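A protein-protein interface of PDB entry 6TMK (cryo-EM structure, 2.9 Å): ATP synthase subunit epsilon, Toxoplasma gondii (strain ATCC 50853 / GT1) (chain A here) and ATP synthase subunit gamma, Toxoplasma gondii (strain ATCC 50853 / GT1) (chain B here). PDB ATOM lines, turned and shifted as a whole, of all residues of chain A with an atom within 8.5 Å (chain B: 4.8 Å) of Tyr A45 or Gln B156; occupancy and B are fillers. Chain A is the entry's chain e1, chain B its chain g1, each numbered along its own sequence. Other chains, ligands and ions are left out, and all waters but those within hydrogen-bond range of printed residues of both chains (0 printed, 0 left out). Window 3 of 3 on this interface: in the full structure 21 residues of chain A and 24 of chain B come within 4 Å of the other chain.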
ATOM      1  N   GLU A  42       6.168  19.376 -12.568  1.00  0.00           N
ATOM      2  CA  GLU A  42       5.330  18.704 -11.590  1.00  0.00           C
ATOM      3  C   GLU A  42       3.951  18.405 -12.168  1.00  0.00           C
ATOM      4  O   GLU A  42       3.401  19.174 -12.964  1.00  0.00           O
ATOM      5  CB  GLU A  42       5.198  19.557 -10.329  1.00  0.00           C
ATOM      6  CG  GLU A  42       4.607  18.827  -9.134  1.00  0.00           C
ATOM      7  CD  GLU A  42       4.164  19.771  -8.032  1.00  0.00           C
ATOM      8  OE1 GLU A  42       4.388  20.992  -8.165  1.00  0.00           O
ATOM      9  OE2 GLU A  42       3.592  19.291  -7.031  1.00  0.00           O
ATOM     10  N   THR A  43       3.395  17.272 -11.743  1.00  0.00           N
ATOM     11  CA  THR A  43       2.143  16.735 -12.270  1.00  0.00           C
ATOM     12  C   THR A  43       1.375  16.119 -11.111  1.00  0.00           C
ATOM     13  O   THR A  43       1.775  15.070 -10.596  1.00  0.00           O
ATOM     14  CB  THR A  43       2.404  15.694 -13.359  1.00  0.00           C
ATOM     15  OG1 THR A  43       3.466  16.143 -14.211  1.00  0.00           O
ATOM     16  CG2 THR A  43       1.157  15.454 -14.180  1.00  0.00           C
ATOM     17  N   VAL A  44       0.280  16.755 -10.697  1.00  0.00           N
ATOM     18  CA  VAL A  44      -0.406  16.393  -9.461  1.00  0.00           C
ATOM     19  C   VAL A  44      -1.617  15.535  -9.787  1.00  0.00           C
ATOM     20  O   VAL A  44      -2.349  15.804 -10.748  1.00  0.00           O
ATOM     21  CB  VAL A  44      -0.827  17.646  -8.672  1.00  0.00           C
ATOM     22  CG1 VAL A  44      -1.336  17.255  -7.297  1.00  0.00           C
ATOM     23  CG2 VAL A  44       0.331  18.616  -8.557  1.00  0.00           C
ATOM     24  N   TYR A  45      -1.824  14.496  -8.983  1.00  0.00           N
ATOM     25  CA  TYR A  45      -2.843  13.489  -9.229  1.00  0.00           C
ATOM     26  C   TYR A  45      -3.732  13.361  -8.001  1.00  0.00           C
ATOM     27  O   TYR A  45      -3.335  13.694  -6.882  1.00  0.00           O
ATOM     28  CB  TYR A  45      -2.220  12.124  -9.548  1.00  0.00           C
ATOM     29  CG  TYR A  45      -1.739  11.972 -10.970  1.00  0.00           C
ATOM     30  CD1 TYR A  45      -0.747  12.798 -11.480  1.00  0.00           C
ATOM     31  CD2 TYR A  45      -2.269  10.996 -11.801  1.00  0.00           C
ATOM     32  CE1 TYR A  45      -0.299  12.656 -12.779  1.00  0.00           C
ATOM     33  CE2 TYR A  45      -1.830  10.848 -13.099  1.00  0.00           C
ATOM     34  CZ  TYR A  45      -0.844  11.679 -13.583  1.00  0.00           C
ATOM     35  OH  TYR A  45      -0.405  11.536 -14.879  1.00  0.00           O
ATOM     36  N   GLN A  46      -4.950  12.871  -8.224  1.00  0.00           N
ATOM     37  CA  GLN A  46      -5.866  12.554  -7.126  1.00  0.00           C
ATOM     38  C   GLN A  46      -6.752  11.401  -7.600  1.00  0.00           C
ATOM     39  O   GLN A  46      -7.805  11.620  -8.204  1.00  0.00           O
ATOM     40  CB  GLN A  46      -6.687  13.765  -6.711  1.00  0.00           C
ATOM     41  CG  GLN A  46      -7.538  13.535  -5.471  1.00  0.00           C
ATOM     42  CD  GLN A  46      -6.709  13.417  -4.205  1.00  0.00           C
ATOM     43  OE1 GLN A  46      -6.112  12.374  -3.938  1.00  0.00           O
ATOM     44  NE2 GLN A  46      -6.669  14.486  -3.419  1.00  0.00           N
ATOM     45  N   GLN A  47      -6.320  10.177  -7.310  1.00  0.00           N
ATOM     46  CA  GLN A  47      -6.974   8.982  -7.831  1.00  0.00           C
ATOM     47  C   GLN A  47      -7.119   9.087  -9.349  1.00  0.00           C
ATOM     48  O   GLN A  47      -8.219   9.121  -9.902  1.00  0.00           O
ATOM     49  CB  GLN A  47      -8.333   8.768  -7.160  1.00  0.00           C
ATOM     50  CG  GLN A  47      -8.927   7.388  -7.398  1.00  0.00           C
ATOM     51  CD  GLN A  47      -9.969   7.375  -8.501  1.00  0.00           C
ATOM     52  OE1 GLN A  47     -10.714   8.338  -8.678  1.00  0.00           O
ATOM     53  NE2 GLN A  47     -10.014   6.284  -9.256  1.00  0.00           N
ATOM     54  N   GLY A  48      -5.974   9.152 -10.020  1.00  0.00           N
ATOM     55  CA  GLY A  48      -6.027   9.575 -11.396  1.00  0.00           C
ATOM     56  C   GLY A  48      -6.499  11.020 -11.441  1.00  0.00           C
ATOM     57  O   GLY A  48      -6.390  11.774 -10.471  1.00  0.00           O
ATOM     58  N   GLN A  49      -7.040  11.403 -12.596  1.00  0.00           N
ATOM     59  CA  GLN A  49      -7.755  12.671 -12.735  1.00  0.00           C
ATOM     60  C   GLN A  49      -6.845  13.836 -12.336  1.00  0.00           C
ATOM     61  O   GLN A  49      -7.017  14.485 -11.303  1.00  0.00           O
ATOM     62  CB  GLN A  49      -9.039  12.666 -11.896  1.00  0.00           C
ATOM     63  CG  GLN A  49      -9.910  11.433 -12.091  1.00  0.00           C
ATOM     64  CD  GLN A  49     -10.614  11.009 -10.817  1.00  0.00           C
ATOM     65  OE1 GLN A  49     -10.671  11.759  -9.843  1.00  0.00           O
ATOM     66  NE2 GLN A  49     -11.142   9.793 -10.815  1.00  0.00           N
ATOM     67  N   VAL A  50      -5.851  14.064 -13.193  1.00  0.00           N
ATOM     68  CA  VAL A  50      -4.842  15.093 -12.975  1.00  0.00           C
ATOM     69  C   VAL A  50      -5.493  16.385 -12.505  1.00  0.00           C
ATOM     70  O   VAL A  50      -6.425  16.893 -13.137  1.00  0.00           O
ATOM     71  CB  VAL A  50      -4.025  15.334 -14.257  1.00  0.00           C
ATOM     72  CG1 VAL A  50      -3.259  16.641 -14.161  1.00  0.00           C
ATOM     73  CG2 VAL A  50      -3.085  14.176 -14.506  1.00  0.00           C
ATOM     74  N   LEU A  51      -5.003  16.924 -11.387  1.00  0.00           N
ATOM     75  CA  LEU A  51      -5.484  18.215 -10.915  1.00  0.00           C
ATOM     76  C   LEU A  51      -4.785  19.361 -11.631  1.00  0.00           C
ATOM     77  O   LEU A  51      -5.421  20.367 -11.965  1.00  0.00           O
ATOM     78  CB  LEU A  51      -5.274  18.339  -9.406  1.00  0.00           C
ATOM     79  CG  LEU A  51      -5.725  17.151  -8.557  1.00  0.00           C
ATOM     80  CD1 LEU A  51      -5.608  17.485  -7.077  1.00  0.00           C
ATOM     81  CD2 LEU A  51      -7.145  16.753  -8.910  1.00  0.00           C
ATOM     82  N   THR A  52      -3.485  19.229 -11.880  1.00  0.00           N
ATOM     83  CA  THR A  52      -2.746  20.292 -12.541  1.00  0.00           C
ATOM     84  C   THR A  52      -1.388  19.767 -12.983  1.00  0.00           C
ATOM     85  O   THR A  52      -0.904  18.736 -12.504  1.00  0.00           O
ATOM     86  CB  THR A  52      -2.568  21.508 -11.625  1.00  0.00           C
ATOM     87  OG1 THR A  52      -1.838  22.529 -12.316  1.00  0.00           O
ATOM     88  CG2 THR A  52      -1.816  21.124 -10.358  1.00  0.00           C
ATOM     89  N   ARG A  53      -0.796  20.493 -13.926  1.00  0.00           N
ATOM     90  CA  ARG A  53       0.572  20.278 -14.369  1.00  0.00           C
ATOM     91  C   ARG A  53       1.233  21.640 -14.493  1.00  0.00           C
ATOM     92  O   ARG A  53       0.612  22.591 -14.976  1.00  0.00           O
ATOM     93  CB  ARG A  53       0.620  19.530 -15.702  1.00  0.00           C
ATOM     94  CG  ARG A  53      -0.443  18.462 -15.825  1.00  0.00           C
ATOM     95  CD  ARG A  53      -0.250  17.617 -17.067  1.00  0.00           C
ATOM     96  NE  ARG A  53      -1.354  16.683 -17.264  1.00  0.00           N
ATOM     97  CZ  ARG A  53      -2.568  17.035 -17.669  1.00  0.00           C
ATOM     98  NH1 ARG A  53      -2.847  18.307 -17.920  1.00  0.00           N
ATOM     99  NH2 ARG A  53      -3.509  16.114 -17.818  1.00  0.00           N
ATOM    100  N   GLU A  54       2.484  21.737 -14.055  1.00  0.00           N
ATOM    101  CA  GLU A  54       3.163  23.024 -14.066  1.00  0.00           C
ATOM    102  C   GLU A  54       4.664  22.828 -14.178  1.00  0.00           C
ATOM    103  O   GLU A  54       5.227  21.910 -13.577  1.00  0.00           O
ATOM    104  CB  GLU A  54       2.830  23.832 -12.808  1.00  0.00           C
ATOM    105  CG  GLU A  54       3.084  23.093 -11.507  1.00  0.00           C
ATOM    106  CD  GLU A  54       1.843  22.411 -10.970  1.00  0.00           C
ATOM    107  OE1 GLU A  54       1.365  22.809  -9.886  1.00  0.00           O
ATOM    108  OE2 GLU A  54       1.347  21.471 -11.626  1.00  0.00           O
ATOM    109  N   ILE B 151       8.189   5.000 -15.176  1.00  0.00           N
ATOM    110  CA  ILE B 151       7.462   4.396 -14.061  1.00  0.00           C
ATOM    111  C   ILE B 151       5.974   4.704 -14.170  1.00  0.00           C
ATOM    112  O   ILE B 151       5.122   3.862 -13.855  1.00  0.00           O
ATOM    113  CB  ILE B 151       8.049   4.881 -12.723  1.00  0.00           C
ATOM    114  CG1 ILE B 151       7.543   4.010 -11.573  1.00  0.00           C
ATOM    115  CG2 ILE B 151       7.708   6.342 -12.485  1.00  0.00           C
ATOM    116  CD1 ILE B 151       8.208   2.657 -11.498  1.00  0.00           C
ATOM    117  N   ARG B 152       5.639   5.912 -14.626  1.00  0.00           N
ATOM    118  CA  ARG B 152       4.239   6.273 -14.807  1.00  0.00           C
ATOM    119  C   ARG B 152       3.580   5.364 -15.833  1.00  0.00           C
ATOM    120  O   ARG B 152       2.503   4.807 -15.590  1.00  0.00           O
ATOM    121  CB  ARG B 152       4.137   7.735 -15.239  1.00  0.00           C
ATOM    122  CG  ARG B 152       2.847   8.092 -15.952  1.00  0.00           C
ATOM    123  CD  ARG B 152       2.612   9.588 -15.928  1.00  0.00           C
ATOM    124  NE  ARG B 152       3.675  10.310 -16.621  1.00  0.00           N
ATOM    125  CZ  ARG B 152       3.662  11.618 -16.860  1.00  0.00           C
ATOM    126  NH1 ARG B 152       2.634  12.362 -16.472  1.00  0.00           N
ATOM    127  NH2 ARG B 152       4.677  12.184 -17.498  1.00  0.00           N
ATOM    128  N   SER B 153       4.218   5.198 -16.990  1.00  0.00           N
ATOM    129  CA  SER B 153       3.666   4.325 -18.018  1.00  0.00           C
ATOM    130  C   SER B 153       3.621   2.876 -17.554  1.00  0.00           C
ATOM    131  O   SER B 153       2.758   2.110 -17.994  1.00  0.00           O
ATOM    132  CB  SER B 153       4.488   4.445 -19.299  1.00  0.00           C
ATOM    133  OG  SER B 153       5.845   4.118 -19.061  1.00  0.00           O
ATOM    134  N   ALA B 154       4.536   2.483 -16.666  1.00  0.00           N
ATOM    135  CA  ALA B 154       4.580   1.102 -16.205  1.00  0.00           C
ATOM    136  C   ALA B 154       3.500   0.796 -15.176  1.00  0.00           C
ATOM    137  O   ALA B 154       3.002  -0.333 -15.132  1.00  0.00           O
ATOM    138  CB  ALA B 154       5.956   0.792 -15.616  1.00  0.00           C
ATOM    139  N   LEU B 155       3.125   1.772 -14.350  1.00  0.00           N
ATOM    140  CA  LEU B 155       2.235   1.522 -13.224  1.00  0.00           C
ATOM    141  C   LEU B 155       0.890   2.224 -13.343  1.00  0.00           C
ATOM    142  O   LEU B 155       0.079   2.135 -12.415  1.00  0.00           O
ATOM    143  CB  LEU B 155       2.913   1.946 -11.917  1.00  0.00           C
ATOM    144  CG  LEU B 155       4.212   1.219 -11.570  1.00  0.00           C
ATOM    145  CD1 LEU B 155       4.816   1.783 -10.300  1.00  0.00           C
ATOM    146  CD2 LEU B 155       3.969  -0.273 -11.426  1.00  0.00           C
ATOM    147  N   GLN B 156       0.627   2.920 -14.448  1.00  0.00           N
ATOM    148  CA  GLN B 156      -0.639   3.618 -14.622  1.00  0.00           C
ATOM    149  C   GLN B 156      -1.812   2.654 -14.506  1.00  0.00           C
ATOM    150  O   GLN B 156      -2.621   2.754 -13.578  1.00  0.00           O
ATOM    151  CB  GLN B 156      -0.674   4.330 -15.977  1.00  0.00           C
ATOM    152  CG  GLN B 156      -1.785   5.357 -16.106  1.00  0.00           C
ATOM    153  CD  GLN B 156      -1.383   6.722 -15.588  1.00  0.00           C
ATOM    154  OE1 GLN B 156      -0.249   7.162 -15.772  1.00  0.00           O
ATOM    155  NE2 GLN B 156      -2.316   7.402 -14.933  1.00  0.00           N
ATOM    156  N   ARG B 157      -1.910   1.715 -15.450  1.00  0.00           N
ATOM    157  CA  ARG B 157      -3.099   0.877 -15.553  1.00  0.00           C
ATOM    158  C   ARG B 157      -3.332   0.057 -14.292  1.00  0.00           C
ATOM    159  O   ARG B 157      -4.477  -0.284 -13.978  1.00  0.00           O
ATOM    160  CB  ARG B 157      -2.975  -0.051 -16.761  1.00  0.00           C
ATOM    161  CG  ARG B 157      -1.956  -1.160 -16.571  1.00  0.00           C
ATOM    162  CD  ARG B 157      -1.272  -1.510 -17.878  1.00  0.00           C
ATOM    163  NE  ARG B 157      -0.566  -2.788 -17.801  1.00  0.00           N
ATOM    164  CZ  ARG B 157      -1.042  -3.949 -18.246  1.00  0.00           C
ATOM    165  NH1 ARG B 157      -2.244  -4.022 -18.802  1.00  0.00           N
ATOM    166  NH2 ARG B 157      -0.313  -5.049 -18.126  1.00  0.00           N
ATOM    167  N   THR B 158      -2.269  -0.265 -13.558  1.00  0.00           N
ATOM    168  CA  THR B 158      -2.353  -1.172 -12.420  1.00  0.00           C
ATOM    169  C   THR B 158      -2.429  -0.447 -11.086  1.00  0.00           C
ATOM    170  O   THR B 158      -3.123  -0.910 -10.175  1.00  0.00           O
ATOM    171  CB  THR B 158      -1.146  -2.115 -12.407  1.00  0.00           C
ATOM    172  OG1 THR B 158      -0.907  -2.614 -13.729  1.00  0.00           O
ATOM    173  CG2 THR B 158      -1.388  -3.279 -11.461  1.00  0.00           C
ATOM    174  N   PHE B 159      -1.733   0.678 -10.946  1.00  0.00           N
ATOM    175  CA  PHE B 159      -1.677   1.410  -9.687  1.00  0.00           C
ATOM    176  C   PHE B 159      -1.791   2.904  -9.942  1.00  0.00           C
ATOM    177  O   PHE B 159      -1.125   3.718  -9.294  1.00  0.00           O
ATOM    178  CB  PHE B 159      -0.394   1.083  -8.924  1.00  0.00           C
ATOM    179  CG  PHE B 159      -0.299  -0.352  -8.493  1.00  0.00           C
ATOM    180  CD1 PHE B 159       0.692  -1.176  -8.995  1.00  0.00           C
ATOM    181  CD2 PHE B 159      -1.205  -0.877  -7.587  1.00  0.00           C
ATOM    182  CE1 PHE B 159       0.781  -2.495  -8.602  1.00  0.00           C
ATOM    183  CE2 PHE B 159      -1.121  -2.196  -7.190  1.00  0.00           C
ATOM    184  CZ  PHE B 159      -0.128  -3.007  -7.698  1.00  0.00           C
ATOM    185  N   GLY B 160      -2.646   3.285 -10.890  1.00  0.00           N
ATOM    186  CA  GLY B 160      -2.917   4.686 -11.145  1.00  0.00           C
ATOM    187  C   GLY B 160      -3.962   5.301 -10.242  1.00  0.00           C
ATOM    188  O   GLY B 160      -4.107   6.526 -10.230  1.00  0.00           O
ATOM    189  N   PHE B 163      -1.593   7.171  -7.392  1.00  0.00           N
ATOM    190  CA  PHE B 163      -0.630   8.235  -7.635  1.00  0.00           C
ATOM    191  C   PHE B 163      -0.938   9.437  -6.752  1.00  0.00           C
ATOM    192  O   PHE B 163      -2.097   9.749  -6.464  1.00  0.00           O
ATOM    193  CB  PHE B 163      -0.656   8.653  -9.106  1.00  0.00           C
ATOM    194  CG  PHE B 163      -0.007   7.666 -10.038  1.00  0.00           C
ATOM    195  CD1 PHE B 163       0.389   6.417  -9.593  1.00  0.00           C
ATOM    196  CD2 PHE B 163       0.189   7.987 -11.368  1.00  0.00           C
ATOM    197  CE1 PHE B 163       0.980   5.516 -10.454  1.00  0.00           C
ATOM    198  CE2 PHE B 163       0.779   7.089 -12.233  1.00  0.00           C
ATOM    199  CZ  PHE B 163       1.174   5.852 -11.775  1.00  0.00           C
ATOM    200  N   LYS B 164       0.121  10.116  -6.324  1.00  0.00           N
ATOM    201  CA  LYS B 164       0.018  11.341  -5.544  1.00  0.00           C
ATOM    202  C   LYS B 164       0.681  12.520  -6.233  1.00  0.00           C
ATOM    203  O   LYS B 164       0.090  13.603  -6.310  1.00  0.00           O
ATOM    204  CB  LYS B 164       0.639  11.123  -4.155  1.00  0.00           C
ATOM    205  CG  LYS B 164       0.450  12.279  -3.189  1.00  0.00           C
ATOM    206  CD  LYS B 164      -1.005  12.467  -2.808  1.00  0.00           C
ATOM    207  CE  LYS B 164      -1.157  13.537  -1.740  1.00  0.00           C
ATOM    208  NZ  LYS B 164      -2.583  13.848  -1.450  1.00  0.00           N
ATOM    209  N   ILE B 166       3.983  13.350  -9.377  1.00  0.00           N
ATOM    210  CA  ILE B 166       4.977  12.836 -10.310  1.00  0.00           C
ATOM    211  C   ILE B 166       5.797  13.996 -10.853  1.00  0.00           C
ATOM    212  O   ILE B 166       5.274  15.093 -11.080  1.00  0.00           O
ATOM    213  CB  ILE B 166       4.318  12.046 -11.455  1.00  0.00           C
ATOM    214  CG1 ILE B 166       3.875  10.678 -10.946  1.00  0.00           C
ATOM    215  CG2 ILE B 166       5.282  11.882 -12.618  1.00  0.00           C
ATOM    216  CD1 ILE B 166       2.715  10.097 -11.696  1.00  0.00           C
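O of Lys B164 is in hydrogen-bond range of N of Tyr A45 (3.4 Å).
The backbone carbonyl oxygen (O) of Gly B160 sits at hydrogen-bond distance from the backbone NH (N) of Gly A48.
The backbone NH (N) of Thr A43 is in hydrogen-bond range of the backbone carbonyl oxygen (O) of Ile B166 (3.0 Å).
The backbone carbonyl oxygen (O) of Glu A54 is in hydrogen-bond range of the backbone NH (N) of Glu A42, 2.9 Å away.
The backbone NH (N) of Gly B160 sits at hydrogen-bond distance from the backbone carbonyl oxygen (O) of Leu B155, 3.3 Å away.
Among the printed residues, pairs that only touch across the chains: Glu A42 with Ile B166 (3.6 Å), Tyr A45 with Arg B152 (3.5 Å), Tyr A45 with Gln B156 (3.9 Å) and Tyr A45 with Phe B163 (3.8 Å).
Gln B156 touches just one residue of chain A: Tyr A45 (3.9 Å).
Of the printed residues of chain A, Arg B152 touches Tyr A45.
Of the printed residues of chain A, Gly B160 touches Gly A48 (3.2 Å).
Val A50 touches none of the printed residues of chain B.
The nearest residue of chain A that does not touch Gln B156 is Gly A48 (5.6 Å).
Of the 13 printed residues of chain B, 6 touch a printed residue of chain A.
Hydrophobic or aromatic side chains of chain B within 4 Å of the printed part of chain A: Phe B163.
Printed residues of chain A that touch a printed residue of chain B: Glu A42, Thr A43, Tyr A45 and Gly A48.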
